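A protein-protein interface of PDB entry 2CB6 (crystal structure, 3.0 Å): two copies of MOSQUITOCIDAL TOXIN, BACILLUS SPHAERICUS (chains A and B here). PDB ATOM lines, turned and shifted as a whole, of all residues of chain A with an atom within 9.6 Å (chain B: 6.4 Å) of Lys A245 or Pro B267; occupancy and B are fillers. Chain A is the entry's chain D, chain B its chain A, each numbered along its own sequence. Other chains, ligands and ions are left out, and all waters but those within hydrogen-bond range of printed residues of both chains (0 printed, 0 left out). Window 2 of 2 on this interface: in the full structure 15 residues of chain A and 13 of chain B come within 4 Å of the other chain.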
ATOM      1  N   ARG A  83      16.427 -19.850 -13.522  1.00  0.00           N
ATOM      2  CA  ARG A  83      15.761 -19.252 -12.373  1.00  0.00           C
ATOM      3  C   ARG A  83      16.495 -19.480 -11.061  1.00  0.00           C
ATOM      4  O   ARG A  83      16.016 -19.060 -10.000  1.00  0.00           O
ATOM      5  CB  ARG A  83      14.324 -19.741 -12.274  1.00  0.00           C
ATOM      6  CG  ARG A  83      13.523 -19.388 -13.502  1.00  0.00           C
ATOM      7  CD  ARG A  83      12.081 -19.107 -13.181  1.00  0.00           C
ATOM      8  NE  ARG A  83      11.413 -18.501 -14.320  1.00  0.00           N
ATOM      9  CZ  ARG A  83      10.849 -17.301 -14.284  1.00  0.00           C
ATOM     10  NH1 ARG A  83      10.879 -16.610 -13.159  1.00  0.00           N
ATOM     11  NH2 ARG A  83      10.256 -16.793 -15.361  1.00  0.00           N
ATOM     12  N   ARG A  84      17.645 -20.147 -11.148  1.00  0.00           N
ATOM     13  CA  ARG A  84      18.483 -20.451  -9.993  1.00  0.00           C
ATOM     14  C   ARG A  84      19.483 -19.317  -9.769  1.00  0.00           C
ATOM     15  O   ARG A  84      20.072 -18.799 -10.722  1.00  0.00           O
ATOM     16  CB  ARG A  84      19.229 -21.770 -10.215  1.00  0.00           C
ATOM     17  CG  ARG A  84      18.313 -22.973 -10.374  1.00  0.00           C
ATOM     18  CD  ARG A  84      19.092 -24.257 -10.613  1.00  0.00           C
ATOM     19  NE  ARG A  84      19.548 -24.378 -11.995  1.00  0.00           N
ATOM     20  CZ  ARG A  84      20.445 -25.268 -12.408  1.00  0.00           C
ATOM     21  NH1 ARG A  84      20.977 -26.116 -11.544  1.00  0.00           N
ATOM     22  NH2 ARG A  84      20.816 -25.305 -13.682  1.00  0.00           N
ATOM     23  N   ASN A 149       8.394 -12.868 -12.137  1.00  0.00           N
ATOM     24  CA  ASN A 149       9.238 -13.238 -11.016  1.00  0.00           C
ATOM     25  C   ASN A 149      10.741 -13.157 -11.245  1.00  0.00           C
ATOM     26  O   ASN A 149      11.222 -12.392 -12.096  1.00  0.00           O
ATOM     27  CB  ASN A 149       8.814 -14.603 -10.483  1.00  0.00           C
ATOM     28  CG  ASN A 149       7.310 -14.696 -10.270  1.00  0.00           C
ATOM     29  OD1 ASN A 149       6.766 -14.084  -9.352  1.00  0.00           O
ATOM     30  ND2 ASN A 149       6.625 -15.412 -11.155  1.00  0.00           N
ATOM     31  N   ILE A 150      11.479 -13.936 -10.454  1.00  0.00           N
ATOM     32  CA  ILE A 150      12.935 -13.948 -10.517  1.00  0.00           C
ATOM     33  C   ILE A 150      13.551 -14.977 -11.454  1.00  0.00           C
ATOM     34  O   ILE A 150      13.452 -16.193 -11.219  1.00  0.00           O
ATOM     35  CB  ILE A 150      13.559 -14.169  -9.140  1.00  0.00           C
ATOM     36  CG1 ILE A 150      13.150 -13.063  -8.183  1.00  0.00           C
ATOM     37  CG2 ILE A 150      15.085 -14.240  -9.246  1.00  0.00           C
ATOM     38  CD1 ILE A 150      13.220 -13.499  -6.749  1.00  0.00           C
ATOM     39  N   MET A 242      15.328 -16.313  -5.304  1.00  0.00           N
ATOM     40  CA  MET A 242      14.681 -17.122  -6.331  1.00  0.00           C
ATOM     41  C   MET A 242      13.228 -17.447  -6.031  1.00  0.00           C
ATOM     42  O   MET A 242      12.789 -17.348  -4.888  1.00  0.00           O
ATOM     43  CB  MET A 242      15.467 -18.403  -6.580  1.00  0.00           C
ATOM     44  CG  MET A 242      15.303 -19.452  -5.514  1.00  0.00           C
ATOM     45  SD  MET A 242      15.879 -21.049  -6.126  1.00  0.00           S
ATOM     46  CE  MET A 242      14.711 -21.391  -7.536  1.00  0.00           C
ATOM     47  N   ASP A 243      12.483 -17.824  -7.065  1.00  0.00           N
ATOM     48  CA  ASP A 243      11.074 -18.153  -6.910  1.00  0.00           C
ATOM     49  C   ASP A 243      10.827 -19.228  -5.858  1.00  0.00           C
ATOM     50  O   ASP A 243      11.604 -20.176  -5.718  1.00  0.00           O
ATOM     51  CB  ASP A 243      10.481 -18.581  -8.246  1.00  0.00           C
ATOM     52  CG  ASP A 243      10.588 -17.508  -9.296  1.00  0.00           C
ATOM     53  OD1 ASP A 243      10.893 -16.359  -8.935  1.00  0.00           O
ATOM     54  OD2 ASP A 243      10.367 -17.822 -10.484  1.00  0.00           O
ATOM     55  N   SER A 244       9.723 -19.068  -5.137  1.00  0.00           N
ATOM     56  CA  SER A 244       9.316 -19.986  -4.074  1.00  0.00           C
ATOM     57  C   SER A 244       9.437 -21.474  -4.410  1.00  0.00           C
ATOM     58  O   SER A 244       9.875 -22.266  -3.573  1.00  0.00           O
ATOM     59  CB  SER A 244       7.888 -19.664  -3.641  1.00  0.00           C
ATOM     60  OG  SER A 244       6.953 -20.186  -4.570  1.00  0.00           O
ATOM     61  N   LYS A 245       9.049 -21.877  -5.616  1.00  0.00           N
ATOM     62  CA  LYS A 245       9.070 -23.297  -5.996  1.00  0.00           C
ATOM     63  C   LYS A 245      10.345 -24.109  -5.775  1.00  0.00           C
ATOM     64  O   LYS A 245      10.301 -25.329  -5.605  1.00  0.00           O
ATOM     65  CB  LYS A 245       8.625 -23.489  -7.435  1.00  0.00           C
ATOM     66  CG  LYS A 245       8.562 -24.926  -7.798  1.00  0.00           C
ATOM     67  CD  LYS A 245       7.771 -25.169  -9.065  1.00  0.00           C
ATOM     68  CE  LYS A 245       7.969 -26.617  -9.484  1.00  0.00           C
ATOM     69  NZ  LYS A 245       8.417 -27.320  -8.299  1.00  0.00           N
ATOM     70  N   GLY A 246      11.488 -23.447  -5.884  1.00  0.00           N
ATOM     71  CA  GLY A 246      12.807 -24.082  -5.766  1.00  0.00           C
ATOM     72  C   GLY A 246      13.169 -24.460  -4.352  1.00  0.00           C
ATOM     73  O   GLY A 246      14.172 -25.131  -4.123  1.00  0.00           O
ATOM     74  N   PHE A 247      12.341 -24.044  -3.395  1.00  0.00           N
ATOM     75  CA  PHE A 247      12.558 -24.371  -1.970  1.00  0.00           C
ATOM     76  C   PHE A 247      11.757 -25.592  -1.547  1.00  0.00           C
ATOM     77  O   PHE A 247      11.902 -26.092  -0.434  1.00  0.00           O
ATOM     78  CB  PHE A 247      12.123 -23.219  -1.081  1.00  0.00           C
ATOM     79  CG  PHE A 247      12.904 -21.994  -1.289  1.00  0.00           C
ATOM     80  CD1 PHE A 247      14.197 -21.919  -0.857  1.00  0.00           C
ATOM     81  CD2 PHE A 247      12.356 -20.906  -1.914  1.00  0.00           C
ATOM     82  CE1 PHE A 247      14.937 -20.784  -1.044  1.00  0.00           C
ATOM     83  CE2 PHE A 247      13.083 -19.767  -2.077  1.00  0.00           C
ATOM     84  CZ  PHE A 247      14.378 -19.700  -1.646  1.00  0.00           C
ATOM     85  N   ILE A 248      10.855 -26.027  -2.417  1.00  0.00           N
ATOM     86  CA  ILE A 248      10.061 -27.195  -2.111  1.00  0.00           C
ATOM     87  C   ILE A 248      10.992 -28.333  -2.485  1.00  0.00           C
ATOM     88  O   ILE A 248      11.239 -28.641  -3.634  1.00  0.00           O
ATOM     89  CB  ILE A 248       8.690 -27.234  -2.798  1.00  0.00           C
ATOM     90  CG1 ILE A 248       7.946 -25.918  -2.557  1.00  0.00           C
ATOM     91  CG2 ILE A 248       7.883 -28.405  -2.275  1.00  0.00           C
ATOM     92  CD1 ILE A 248       6.796 -25.646  -3.513  1.00  0.00           C
ATOM     93  N   LEU A 249      11.630 -28.873  -1.469  1.00  0.00           N
ATOM     94  CA  LEU A 249      12.639 -29.874  -1.722  1.00  0.00           C
ATOM     95  C   LEU A 249      12.100 -31.255  -2.046  1.00  0.00           C
ATOM     96  O   LEU A 249      12.753 -32.017  -2.767  1.00  0.00           O
ATOM     97  CB  LEU A 249      13.667 -29.927  -0.590  1.00  0.00           C
ATOM     98  CG  LEU A 249      14.805 -28.896  -0.569  1.00  0.00           C
ATOM     99  CD1 LEU A 249      14.330 -27.452  -0.763  1.00  0.00           C
ATOM    100  CD2 LEU A 249      15.505 -29.013   0.767  1.00  0.00           C
ATOM    101  N   ASP A 250      10.924 -31.583  -1.510  1.00  0.00           N
ATOM    102  CA  ASP A 250      10.286 -32.874  -1.759  1.00  0.00           C
ATOM    103  C   ASP A 250       9.981 -32.983  -3.273  1.00  0.00           C
ATOM    104  O   ASP A 250       9.962 -34.084  -3.834  1.00  0.00           O
ATOM    105  CB  ASP A 250       8.969 -32.998  -0.944  1.00  0.00           C
ATOM    106  CG  ASP A 250       9.118 -32.543   0.536  1.00  0.00           C
ATOM    107  OD1 ASP A 250       9.521 -33.373   1.409  1.00  0.00           O
ATOM    108  OD2 ASP A 250       8.786 -31.360   0.835  1.00  0.00           O
ATOM    109  N   LEU A 251       9.757 -31.827  -3.909  1.00  0.00           N
ATOM    110  CA  LEU A 251       9.428 -31.723  -5.344  1.00  0.00           C
ATOM    111  C   LEU A 251      10.591 -31.453  -6.274  1.00  0.00           C
ATOM    112  O   LEU A 251      11.336 -30.511  -6.107  1.00  0.00           O
ATOM    113  CB  LEU A 251       8.454 -30.580  -5.567  1.00  0.00           C
ATOM    114  CG  LEU A 251       7.035 -30.605  -5.007  1.00  0.00           C
ATOM    115  CD1 LEU A 251       6.234 -29.440  -5.539  1.00  0.00           C
ATOM    116  CD2 LEU A 251       6.327 -31.942  -5.224  1.00  0.00           C
ATOM    117  N   ASP A 252      10.690 -32.259  -7.329  1.00  0.00           N
ATOM    118  CA  ASP A 252      11.749 -32.072  -8.313  1.00  0.00           C
ATOM    119  C   ASP A 252      11.743 -30.857  -9.243  1.00  0.00           C
ATOM    120  O   ASP A 252      10.694 -30.408  -9.757  1.00  0.00           O
ATOM    121  CB  ASP A 252      12.428 -33.348  -8.822  1.00  0.00           C
ATOM    122  CG  ASP A 252      11.506 -34.202  -9.657  1.00  0.00           C
ATOM    123  OD1 ASP A 252      10.650 -33.611 -10.326  1.00  0.00           O
ATOM    124  OD2 ASP A 252      11.597 -35.452  -9.635  1.00  0.00           O
ATOM    125  N   TYR A 253      12.947 -30.318  -9.414  1.00  0.00           N
ATOM    126  CA  TYR A 253      13.148 -29.100 -10.152  1.00  0.00           C
ATOM    127  C   TYR A 253      13.372 -29.206 -11.645  1.00  0.00           C
ATOM    128  O   TYR A 253      14.347 -29.799 -12.109  1.00  0.00           O
ATOM    129  CB  TYR A 253      14.214 -28.234  -9.444  1.00  0.00           C
ATOM    130  CG  TYR A 253      14.035 -26.748  -9.666  1.00  0.00           C
ATOM    131  CD1 TYR A 253      12.970 -26.059  -9.105  1.00  0.00           C
ATOM    132  CD2 TYR A 253      14.906 -26.043 -10.503  1.00  0.00           C
ATOM    133  CE1 TYR A 253      12.780 -24.733  -9.350  1.00  0.00           C
ATOM    134  CE2 TYR A 253      14.720 -24.695 -10.758  1.00  0.00           C
ATOM    135  CZ  TYR A 253      13.639 -24.044 -10.187  1.00  0.00           C
ATOM    136  OH  TYR A 253      13.420 -22.700 -10.416  1.00  0.00           O
ATOM    137  N   ASN A 254      12.477 -28.593 -12.414  1.00  0.00           N
ATOM    138  CA  ASN A 254      12.721 -28.578 -13.845  1.00  0.00           C
ATOM    139  C   ASN A 254      13.374 -27.256 -14.179  1.00  0.00           C
ATOM    140  O   ASN A 254      12.726 -26.239 -14.502  1.00  0.00           O
ATOM    141  CB  ASN A 254      11.533 -28.809 -14.723  1.00  0.00           C
ATOM    142  CG  ASN A 254      11.975 -28.949 -16.129  1.00  0.00           C
ATOM    143  OD1 ASN A 254      13.166 -29.179 -16.371  1.00  0.00           O
ATOM    144  ND2 ASN A 254      11.052 -28.810 -17.073  1.00  0.00           N
ATOM    145  N   GLN A 255      14.682 -27.313 -14.085  1.00  0.00           N
ATOM    146  CA  GLN A 255      15.564 -26.164 -14.200  1.00  0.00           C
ATOM    147  C   GLN A 255      15.865 -25.824 -15.645  1.00  0.00           C
ATOM    148  O   GLN A 255      16.350 -24.724 -15.942  1.00  0.00           O
ATOM    149  CB  GLN A 255      16.881 -26.469 -13.494  1.00  0.00           C
ATOM    150  CG  GLN A 255      17.655 -27.580 -14.153  1.00  0.00           C
ATOM    151  CD  GLN A 255      18.323 -28.491 -13.159  1.00  0.00           C
ATOM    152  OE1 GLN A 255      17.684 -28.977 -12.226  1.00  0.00           O
ATOM    153  NE2 GLN A 255      19.610 -28.751 -13.363  1.00  0.00           N
ATOM    154  N   PHE A 257      13.613 -25.782 -17.869  1.00  0.00           N
ATOM    155  CA  PHE A 257      12.353 -25.318 -18.425  1.00  0.00           C
ATOM    156  C   PHE A 257      12.386 -24.093 -19.329  1.00  0.00           C
ATOM    157  O   PHE A 257      11.825 -24.107 -20.420  1.00  0.00           O
ATOM    158  CB  PHE A 257      11.293 -25.156 -17.338  1.00  0.00           C
ATOM    159  CG  PHE A 257       9.931 -24.808 -17.873  1.00  0.00           C
ATOM    160  CD1 PHE A 257       8.992 -25.794 -18.126  1.00  0.00           C
ATOM    161  CD2 PHE A 257       9.595 -23.488 -18.150  1.00  0.00           C
ATOM    162  CE1 PHE A 257       7.740 -25.472 -18.636  1.00  0.00           C
ATOM    163  CE2 PHE A 257       8.340 -23.164 -18.649  1.00  0.00           C
ATOM    164  CZ  PHE A 257       7.416 -24.160 -18.892  1.00  0.00           C
ATOM    165  N   THR B 139      -2.828 -28.774  -4.875  1.00  0.00           N
ATOM    166  CA  THR B 139      -2.521 -28.922  -6.292  1.00  0.00           C
ATOM    167  C   THR B 139      -1.893 -30.258  -6.670  1.00  0.00           C
ATOM    168  O   THR B 139      -0.953 -30.727  -6.021  1.00  0.00           O
ATOM    169  CB  THR B 139      -1.678 -27.755  -6.830  1.00  0.00           C
ATOM    170  OG1 THR B 139      -2.233 -26.507  -6.379  1.00  0.00           O
ATOM    171  CG2 THR B 139      -1.679 -27.776  -8.352  1.00  0.00           C
ATOM    172  N   PRO B 140      -2.430 -30.873  -7.719  1.00  0.00           N
ATOM    173  CA  PRO B 140      -1.926 -32.153  -8.207  1.00  0.00           C
ATOM    174  C   PRO B 140      -0.954 -31.913  -9.365  1.00  0.00           C
ATOM    175  O   PRO B 140      -0.800 -30.774  -9.820  1.00  0.00           O
ATOM    176  CB  PRO B 140      -3.196 -32.822  -8.749  1.00  0.00           C
ATOM    177  CG  PRO B 140      -4.010 -31.676  -9.269  1.00  0.00           C
ATOM    178  CD  PRO B 140      -3.685 -30.482  -8.395  1.00  0.00           C
ATOM    179  N   TRP B 141      -0.313 -32.980  -9.847  1.00  0.00           N
ATOM    180  CA  TRP B 141       0.584 -32.869 -10.985  1.00  0.00           C
ATOM    181  C   TRP B 141      -0.267 -32.230 -12.081  1.00  0.00           C
ATOM    182  O   TRP B 141      -1.381 -32.666 -12.344  1.00  0.00           O
ATOM    183  CB  TRP B 141       1.047 -34.258 -11.409  1.00  0.00           C
ATOM    184  CG  TRP B 141       2.008 -34.280 -12.583  1.00  0.00           C
ATOM    185  CD1 TRP B 141       3.379 -34.361 -12.523  1.00  0.00           C
ATOM    186  CD2 TRP B 141       1.669 -34.257 -13.982  1.00  0.00           C
ATOM    187  NE1 TRP B 141       3.907 -34.375 -13.798  1.00  0.00           N
ATOM    188  CE2 TRP B 141       2.881 -34.303 -14.708  1.00  0.00           C
ATOM    189  CE3 TRP B 141       0.463 -34.179 -14.689  1.00  0.00           C
ATOM    190  CZ2 TRP B 141       2.918 -34.280 -16.103  1.00  0.00           C
ATOM    191  CZ3 TRP B 141       0.503 -34.170 -16.066  1.00  0.00           C
ATOM    192  CH2 TRP B 141       1.720 -34.221 -16.760  1.00  0.00           C
ATOM    193  N   THR B 142       0.214 -31.144 -12.662  1.00  0.00           N
ATOM    194  CA  THR B 142      -0.573 -30.455 -13.667  1.00  0.00           C
ATOM    195  C   THR B 142       0.180 -30.213 -14.966  1.00  0.00           C
ATOM    196  O   THR B 142       1.339 -29.796 -14.960  1.00  0.00           O
ATOM    197  CB  THR B 142      -1.082 -29.108 -13.130  1.00  0.00           C
ATOM    198  OG1 THR B 142      -1.700 -29.295 -11.853  1.00  0.00           O
ATOM    199  CG2 THR B 142      -2.077 -28.507 -14.080  1.00  0.00           C
ATOM    200  N   GLU B 265       4.017 -30.981 -14.129  1.00  0.00           N
ATOM    201  CA  GLU B 265       4.701 -31.094 -12.850  1.00  0.00           C
ATOM    202  C   GLU B 265       3.749 -30.654 -11.753  1.00  0.00           C
ATOM    203  O   GLU B 265       2.690 -30.095 -12.036  1.00  0.00           O
ATOM    204  CB  GLU B 265       5.907 -30.158 -12.837  1.00  0.00           C
ATOM    205  CG  GLU B 265       5.524 -28.686 -12.651  1.00  0.00           C
ATOM    206  CD  GLU B 265       6.698 -27.726 -12.768  1.00  0.00           C
ATOM    207  OE1 GLU B 265       7.843 -28.177 -13.016  1.00  0.00           O
ATOM    208  OE2 GLU B 265       6.465 -26.509 -12.626  1.00  0.00           O
ATOM    209  N   ILE B 266       4.143 -30.884 -10.502  1.00  0.00           N
ATOM    210  CA  ILE B 266       3.346 -30.452  -9.359  1.00  0.00           C
ATOM    211  C   ILE B 266       3.763 -29.011  -9.092  1.00  0.00           C
ATOM    212  O   ILE B 266       4.809 -28.757  -8.497  1.00  0.00           O
ATOM    213  CB  ILE B 266       3.648 -31.284  -8.115  1.00  0.00           C
ATOM    214  CG1 ILE B 266       3.157 -32.715  -8.310  1.00  0.00           C
ATOM    215  CG2 ILE B 266       2.999 -30.654  -6.903  1.00  0.00           C
ATOM    216  CD1 ILE B 266       3.577 -33.658  -7.220  1.00  0.00           C
ATOM    217  N   PRO B 267       2.969 -28.069  -9.580  1.00  0.00           N
ATOM    218  CA  PRO B 267       3.291 -26.653  -9.448  1.00  0.00           C
ATOM    219  C   PRO B 267       3.554 -26.125  -8.037  1.00  0.00           C
ATOM    220  O   PRO B 267       4.474 -25.331  -7.831  1.00  0.00           O
ATOM    221  CB  PRO B 267       2.078 -25.957 -10.068  1.00  0.00           C
ATOM    222  CG  PRO B 267       0.976 -26.917  -9.928  1.00  0.00           C
ATOM    223  CD  PRO B 267       1.576 -28.286 -10.005  1.00  0.00           C
ATOM    224  N   ASN B 268       2.736 -26.550  -7.077  1.00  0.00           N
ATOM    225  CA  ASN B 268       2.863 -26.076  -5.705  1.00  0.00           C
ATOM    226  C   ASN B 268       2.122 -26.999  -4.746  1.00  0.00           C
ATOM    227  O   ASN B 268       1.604 -28.042  -5.150  1.00  0.00           O
ATOM    228  CB  ASN B 268       2.244 -24.684  -5.615  1.00  0.00           C
ATOM    229  CG  ASN B 268       0.816 -24.663  -6.102  1.00  0.00           C
ATOM    230  OD1 ASN B 268      -0.009 -25.471  -5.660  1.00  0.00           O
ATOM    231  ND2 ASN B 268       0.518 -23.768  -7.035  1.00  0.00           N
ATOM    232  N   ASN B 269       2.045 -26.591  -3.481  1.00  0.00           N
ATOM    233  CA  ASN B 269       1.352 -27.380  -2.472  1.00  0.00           C
ATOM    234  C   ASN B 269       0.204 -26.598  -1.858  1.00  0.00           C
ATOM    235  O   ASN B 269      -0.268 -26.909  -0.763  1.00  0.00           O
ATOM    236  CB  ASN B 269       2.328 -27.879  -1.414  1.00  0.00           C
ATOM    237  CG  ASN B 269       3.279 -28.909  -1.968  1.00  0.00           C
ATOM    238  OD1 ASN B 269       3.092 -29.385  -3.083  1.00  0.00           O
ATOM    239  ND2 ASN B 269       4.311 -29.247  -1.210  1.00  0.00           N
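The backbone NH (N) of Thr B142 is in hydrogen-bond range of the backbone carbonyl oxygen (O) of Glu B265, 2.8 Å away.
Glu B265 touches Lys A245 (OE2 to CE, 3.5 Å).
Ile B266 touches Lys A245 (O to NZ, 3.9 Å).
O of Pro B267 touches CD of Lys A245 (3.5 Å).
CG2 of Ile A248 touches ND2 of Asn B269, 3.8 Å away.
Leu A251 touches Ile B266.
Leu A251 touches Asn B269 (CD1 to OD1, 3.99 Å).
Lys A245 touches just these residues of chain B: Glu B265, Ile B266 and Pro B267.
Pro B267 touches just one residue of chain A: Lys A245.
No residue of chain A comes within 4 Å of Thr B142.
Printed residues of chain A within 4 Å of Glu B265: Lys A245 (3.5 Å).
No residue of chain A comes within 4 Å of Asn B268.
Of the printed residues of chain A, Ile B266 touches Lys A245 (3.9 Å) and Leu A251 (3.4 Å).
Of the printed residues of chain B, Leu A251 touches Ile B266 and Asn B269.
The nearest residue of chain B that does not touch Lys A245 is Asn B268 (5.6 Å).
Among the printed residues, no Asp or Glu carboxylate lies within 4 Å of a Lys or Arg side-chain nitrogen of the other chain.
No position is printed for both chains.
Of the 6 pairs that touch across the chains among the printed residues, none has its exchanged pair printed and touching as well.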
